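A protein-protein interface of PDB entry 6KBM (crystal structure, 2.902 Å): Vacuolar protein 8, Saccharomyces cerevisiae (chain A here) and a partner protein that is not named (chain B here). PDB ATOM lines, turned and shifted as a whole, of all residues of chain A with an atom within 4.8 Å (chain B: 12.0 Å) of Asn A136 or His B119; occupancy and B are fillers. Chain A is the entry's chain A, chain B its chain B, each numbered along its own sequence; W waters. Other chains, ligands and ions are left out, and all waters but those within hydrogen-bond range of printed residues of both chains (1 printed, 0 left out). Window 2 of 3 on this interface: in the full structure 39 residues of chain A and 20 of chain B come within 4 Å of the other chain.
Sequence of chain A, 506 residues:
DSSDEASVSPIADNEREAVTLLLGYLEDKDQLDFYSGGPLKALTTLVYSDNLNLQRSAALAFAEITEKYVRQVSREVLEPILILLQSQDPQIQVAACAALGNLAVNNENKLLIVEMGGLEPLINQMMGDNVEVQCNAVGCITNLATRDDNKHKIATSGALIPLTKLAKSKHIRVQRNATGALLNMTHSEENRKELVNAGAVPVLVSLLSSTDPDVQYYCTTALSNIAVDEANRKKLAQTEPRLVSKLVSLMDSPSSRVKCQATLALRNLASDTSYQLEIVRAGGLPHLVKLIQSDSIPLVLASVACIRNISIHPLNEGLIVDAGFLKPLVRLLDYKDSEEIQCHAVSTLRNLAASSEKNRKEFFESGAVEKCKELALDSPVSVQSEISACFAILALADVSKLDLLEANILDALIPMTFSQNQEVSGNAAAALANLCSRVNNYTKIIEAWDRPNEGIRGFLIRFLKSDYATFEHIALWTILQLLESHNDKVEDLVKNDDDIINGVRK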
ATOM      1  N   VAL A  94      23.124   2.230   5.988  1.00  0.00           N
ATOM      2  CA  VAL A  94      22.593   0.900   6.275  1.00  0.00           C
ATOM      3  C   VAL A  94      21.448   0.531   5.337  1.00  0.00           C
ATOM      4  O   VAL A  94      21.517  -0.473   4.622  1.00  0.00           O
ATOM      5  CB  VAL A  94      22.086   0.794   7.728  1.00  0.00           C
ATOM      6  CG1 VAL A  94      21.377  -0.535   7.947  1.00  0.00           C
ATOM      7  CG2 VAL A  94      23.232   0.962   8.710  1.00  0.00           C
ATOM      8  N   CYS A  97      22.440   0.380   1.535  1.00  0.00           N
ATOM      9  CA  CYS A  97      23.192  -0.838   1.257  1.00  0.00           C
ATOM     10  C   CYS A  97      22.274  -2.055   1.230  1.00  0.00           C
ATOM     11  O   CYS A  97      22.302  -2.831   0.280  1.00  0.00           O
ATOM     12  CB  CYS A  97      24.306  -1.036   2.284  1.00  0.00           C
ATOM     13  SG  CYS A  97      25.675   0.125   2.109  1.00  0.00           S
ATOM     14  N   ALA A  98      21.452  -2.209   2.265  1.00  0.00           N
ATOM     15  CA  ALA A  98      20.518  -3.331   2.331  1.00  0.00           C
ATOM     16  C   ALA A  98      19.621  -3.387   1.095  1.00  0.00           C
ATOM     17  O   ALA A  98      19.360  -4.462   0.553  1.00  0.00           O
ATOM     18  CB  ALA A  98      19.677  -3.245   3.591  1.00  0.00           C
ATOM     19  N   GLU A 132      27.241  -2.060  11.350  1.00  0.00           N
ATOM     20  CA  GLU A 132      26.056  -2.356  10.547  1.00  0.00           C
ATOM     21  C   GLU A 132      26.303  -2.141   9.053  1.00  0.00           C
ATOM     22  O   GLU A 132      25.940  -2.987   8.224  1.00  0.00           O
ATOM     23  CB  GLU A 132      24.871  -1.500  11.008  1.00  0.00           C
ATOM     24  CG  GLU A 132      24.256  -1.929  12.337  1.00  0.00           C
ATOM     25  CD  GLU A 132      25.031  -1.430  13.547  1.00  0.00           C
ATOM     26  OE1 GLU A 132      26.147  -0.897  13.371  1.00  0.00           O
ATOM     27  OE2 GLU A 132      24.518  -1.570  14.679  1.00  0.00           O
ATOM     28  N   VAL A 133      26.931  -1.020   8.710  1.00  0.00           N
ATOM     29  CA  VAL A 133      27.205  -0.714   7.312  1.00  0.00           C
ATOM     30  C   VAL A 133      28.288  -1.639   6.764  1.00  0.00           C
ATOM     31  O   VAL A 133      28.314  -1.920   5.566  1.00  0.00           O
ATOM     32  CB  VAL A 133      27.620   0.769   7.104  1.00  0.00           C
ATOM     33  CG1 VAL A 133      26.609   1.699   7.750  1.00  0.00           C
ATOM     34  CG2 VAL A 133      29.016   1.039   7.642  1.00  0.00           C
ATOM     35  N   GLN A 134      29.171  -2.122   7.636  1.00  0.00           N
ATOM     36  CA  GLN A 134      30.155  -3.120   7.235  1.00  0.00           C
ATOM     37  C   GLN A 134      29.428  -4.382   6.804  1.00  0.00           C
ATOM     38  O   GLN A 134      29.608  -4.865   5.685  1.00  0.00           O
ATOM     39  CB  GLN A 134      31.131  -3.434   8.371  1.00  0.00           C
ATOM     40  CG  GLN A 134      32.257  -2.431   8.526  1.00  0.00           C
ATOM     41  CD  GLN A 134      33.182  -2.770   9.679  1.00  0.00           C
ATOM     42  OE1 GLN A 134      32.880  -3.640  10.498  1.00  0.00           O
ATOM     43  NE2 GLN A 134      34.318  -2.086   9.747  1.00  0.00           N
ATOM     44  N   CYS A 135      28.596  -4.894   7.706  1.00  0.00           N
ATOM     45  CA  CYS A 135      27.783  -6.076   7.454  1.00  0.00           C
ATOM     46  C   CYS A 135      27.005  -5.972   6.146  1.00  0.00           C
ATOM     47  O   CYS A 135      27.081  -6.863   5.292  1.00  0.00           O
ATOM     48  CB  CYS A 135      26.818  -6.304   8.618  1.00  0.00           C
ATOM     49  SG  CYS A 135      25.408  -7.365   8.234  1.00  0.00           S
ATOM     50  N   ASN A 136      26.274  -4.875   5.980  1.00  0.00           N
ATOM     51  CA  ASN A 136      25.432  -4.721   4.799  1.00  0.00           C
ATOM     52  C   ASN A 136      26.213  -4.522   3.495  1.00  0.00           C
ATOM     53  O   ASN A 136      25.879  -5.132   2.477  1.00  0.00           O
ATOM     54  CB  ASN A 136      24.453  -3.565   5.002  1.00  0.00           C
ATOM     55  CG  ASN A 136      23.245  -3.973   5.821  1.00  0.00           C
ATOM     56  OD1 ASN A 136      23.241  -5.026   6.455  1.00  0.00           O
ATOM     57  ND2 ASN A 136      22.209  -3.143   5.804  1.00  0.00           N
ATOM     58  N   ALA A 137      27.245  -3.684   3.519  1.00  0.00           N
ATOM     59  CA  ALA A 137      28.036  -3.430   2.312  1.00  0.00           C
ATOM     60  C   ALA A 137      28.767  -4.691   1.859  1.00  0.00           C
ATOM     61  O   ALA A 137      28.742  -5.056   0.670  1.00  0.00           O
ATOM     62  CB  ALA A 137      29.027  -2.301   2.550  1.00  0.00           C
ATOM     63  N   VAL A 138      29.419  -5.350   2.813  1.00  0.00           N
ATOM     64  CA  VAL A 138      30.059  -6.630   2.548  1.00  0.00           C
ATOM     65  C   VAL A 138      29.036  -7.600   1.977  1.00  0.00           C
ATOM     66  O   VAL A 138      29.320  -8.310   1.018  1.00  0.00           O
ATOM     67  CB  VAL A 138      30.695  -7.230   3.813  1.00  0.00           C
ATOM     68  CG1 VAL A 138      31.045  -8.684   3.591  1.00  0.00           C
ATOM     69  CG2 VAL A 138      31.931  -6.452   4.197  1.00  0.00           C
ATOM     70  N   GLY A 139      27.838  -7.610   2.561  1.00  0.00           N
ATOM     71  CA  GLY A 139      26.750  -8.427   2.051  1.00  0.00           C
ATOM     72  C   GLY A 139      26.472  -8.159   0.584  1.00  0.00           C
ATOM     73  O   GLY A 139      26.273  -9.087  -0.209  1.00  0.00           O
ATOM     74  N   CYS A 140      26.465  -6.880   0.221  1.00  0.00           N
ATOM     75  CA  CYS A 140      26.305  -6.489  -1.173  1.00  0.00           C
ATOM     76  C   CYS A 140      27.388  -7.117  -2.037  1.00  0.00           C
ATOM     77  O   CYS A 140      27.088  -7.711  -3.071  1.00  0.00           O
ATOM     78  CB  CYS A 140      26.338  -4.969  -1.323  1.00  0.00           C
ATOM     79  SG  CYS A 140      24.840  -4.138  -0.785  1.00  0.00           S
ATOM     80  N   ARG A 173      28.038 -11.423  12.212  1.00  0.00           N
ATOM     81  CA  ARG A 173      27.302 -11.132  10.984  1.00  0.00           C
ATOM     82  C   ARG A 173      28.273 -10.695   9.888  1.00  0.00           C
ATOM     83  O   ARG A 173      28.244 -11.204   8.752  1.00  0.00           O
ATOM     84  CB  ARG A 173      26.246 -10.055  11.240  1.00  0.00           C
ATOM     85  CG  ARG A 173      25.214 -10.446  12.291  1.00  0.00           C
ATOM     86  CD  ARG A 173      24.205  -9.334  12.542  1.00  0.00           C
ATOM     87  NE  ARG A 173      23.529  -8.908  11.320  1.00  0.00           N
ATOM     88  CZ  ARG A 173      22.358  -9.383  10.907  1.00  0.00           C
ATOM     89  NH1 ARG A 173      21.725 -10.306  11.618  1.00  0.00           N
ATOM     90  NH2 ARG A 173      21.819  -8.933   9.783  1.00  0.00           N
ATOM     91  N   ALA B 114      27.393 -18.616  -1.710  1.00  0.00           N
ATOM     92  CA  ALA B 114      26.960 -18.005  -0.457  1.00  0.00           C
ATOM     93  C   ALA B 114      25.906 -16.922  -0.670  1.00  0.00           C
ATOM     94  O   ALA B 114      25.933 -16.196  -1.662  1.00  0.00           O
ATOM     95  CB  ALA B 114      28.156 -17.432   0.285  1.00  0.00           C
ATOM     96  N   GLN B 115      24.977 -16.827   0.277  1.00  0.00           N
ATOM     97  CA  GLN B 115      23.936 -15.806   0.254  1.00  0.00           C
ATOM     98  C   GLN B 115      24.124 -14.816   1.399  1.00  0.00           C
ATOM     99  O   GLN B 115      24.402 -15.210   2.533  1.00  0.00           O
ATOM    100  CB  GLN B 115      22.550 -16.449   0.340  1.00  0.00           C
ATOM    101  CG  GLN B 115      22.034 -17.005  -0.974  1.00  0.00           C
ATOM    102  CD  GLN B 115      21.170 -16.011  -1.723  1.00  0.00           C
ATOM    103  OE1 GLN B 115      21.104 -14.835  -1.362  1.00  0.00           O
ATOM    104  NE2 GLN B 115      20.499 -16.478  -2.770  1.00  0.00           N
ATOM    105  N   ALA B 116      23.968 -13.532   1.100  1.00  0.00           N
ATOM    106  CA  ALA B 116      24.156 -12.488   2.098  1.00  0.00           C
ATOM    107  C   ALA B 116      22.940 -12.339   3.001  1.00  0.00           C
ATOM    108  O   ALA B 116      21.804 -12.525   2.568  1.00  0.00           O
ATOM    109  CB  ALA B 116      24.464 -11.170   1.423  1.00  0.00           C
ATOM    110  N   LYS B 117      23.194 -12.001   4.261  1.00  0.00           N
ATOM    111  CA  LYS B 117      22.132 -11.726   5.220  1.00  0.00           C
ATOM    112  C   LYS B 117      22.205 -10.268   5.657  1.00  0.00           C
ATOM    113  O   LYS B 117      23.288  -9.752   5.932  1.00  0.00           O
ATOM    114  CB  LYS B 117      22.239 -12.655   6.430  1.00  0.00           C
ATOM    115  CG  LYS B 117      21.203 -13.766   6.446  1.00  0.00           C
ATOM    116  CD  LYS B 117      19.851 -13.270   5.953  1.00  0.00           C
ATOM    117  CE  LYS B 117      18.926 -14.428   5.615  1.00  0.00           C
ATOM    118  NZ  LYS B 117      17.739 -13.973   4.839  1.00  0.00           N
ATOM    119  N   PHE B 118      21.055  -9.603   5.716  1.00  0.00           N
ATOM    120  CA  PHE B 118      21.033  -8.172   5.997  1.00  0.00           C
ATOM    121  C   PHE B 118      20.322  -7.813   7.297  1.00  0.00           C
ATOM    122  O   PHE B 118      19.775  -8.676   7.982  1.00  0.00           O
ATOM    123  CB  PHE B 118      20.384  -7.421   4.835  1.00  0.00           C
ATOM    124  CG  PHE B 118      21.173  -7.484   3.563  1.00  0.00           C
ATOM    125  CD1 PHE B 118      22.350  -6.768   3.430  1.00  0.00           C
ATOM    126  CD2 PHE B 118      20.742  -8.261   2.502  1.00  0.00           C
ATOM    127  CE1 PHE B 118      23.084  -6.825   2.263  1.00  0.00           C
ATOM    128  CE2 PHE B 118      21.471  -8.321   1.332  1.00  0.00           C
ATOM    129  CZ  PHE B 118      22.643  -7.603   1.212  1.00  0.00           C
ATOM    130  N   HIS B 119      20.351  -6.523   7.617  1.00  0.00           N
ATOM    131  CA  HIS B 119      19.737  -5.973   8.823  1.00  0.00           C
ATOM    132  C   HIS B 119      18.272  -6.375   8.962  1.00  0.00           C
ATOM    133  O   HIS B 119      17.860  -6.909   9.993  1.00  0.00           O
ATOM    134  CB  HIS B 119      19.868  -4.445   8.815  1.00  0.00           C
ATOM    135  CG  HIS B 119      19.149  -3.763   9.935  1.00  0.00           C
ATOM    136  ND1 HIS B 119      17.791  -3.522   9.914  1.00  0.00           N
ATOM    137  CD2 HIS B 119      19.601  -3.253  11.107  1.00  0.00           C
ATOM    138  CE1 HIS B 119      17.437  -2.902  11.026  1.00  0.00           C
ATOM    139  NE2 HIS B 119      18.516  -2.727  11.766  1.00  0.00           N
HETATM  140  O   HOH W   1      25.040 -11.583   8.133  1.00  0.00           O
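The side-chain amide oxygen (OD1) of Asn A136 sits at hydrogen-bond distance from the backbone NH (N) of His B119. The guanidinium group (NH2) of Arg A173 sits at hydrogen-bond distance from the backbone carbonyl oxygen (O) of Phe B118 (2.7 Å).
The side-chain amide nitrogen (ND2) of Asn A136 sits at hydrogen-bond distance from the backbone carbonyl oxygen (O) of Val A94 (3.0 Å). The side-chain amide oxygen of Asn A136 lies within hydrogen-bond range of the side-chain sulfur of Cys A135 (3.7 Å). The backbone carbonyl oxygen of Asn A136 sits at hydrogen-bond distance from the side-chain sulfur of Cys A140 (3.6 Å). O of Cys A97 is in hydrogen-bond range of SG of Cys A140 (3.0 Å).
Cys A135 touches Lys B117. Phe B118 touches Asn A136 (CE1 to O, 3.3 Å). Gly A139 touches Ala B116 (O to CB, 3.2 Å). Phe B118 touches Gly A139 (CZ to C, 3.9 Å). Phe B118 touches Cys A140. NH2 of Arg A173 touches N of His B119, 3.6 Å away.
No residue of chain B comes within 4 Å of Val A94. No residue of chain B comes within 4 Å of Ala A98. Of chain B, only Lys B117 (3.9 Å) comes within 4 Å of Cys A135. Asn A136 touches just these residues of chain B: Phe B118 (3.3 Å) and His B119 (3.5 Å). No residue of chain B comes within 4 Å of Ala A137. Gly A139 touches two residues of chain B. Of the printed residues of chain B, Arg A173 touches Phe B118 (2.7 Å) and His B119 (3.6 Å). Gln B115 touches none of the printed residues of chain A. Of the printed residues of chain A, Ala B116 touches Gly A139 (3.2 Å). Printed residues of chain A within 4 Å of Phe B118: Asn A136 (3.3 Å), Gly A139 (3.9 Å), Cys A140 (3.95 Å) and Arg A173 (2.7 Å). His B119 touches two residues of chain A. The nearest residue of chain B that does not touch Asn A136 is Lys B117 (4.8 Å). The nearest printed residue of chain B that does not touch Arg A173 is Lys B117 (4.2 Å).
Hydrophobic or aromatic side chains of chain B within 4 Å of the printed part of chain A: Ala B116 and Phe B118. Among the printed residues, 8 pairs touch across the chains.
Water W1 bridges O of Arg A173 (3.3 Å) and O of Lys B117 (3.4 Å).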
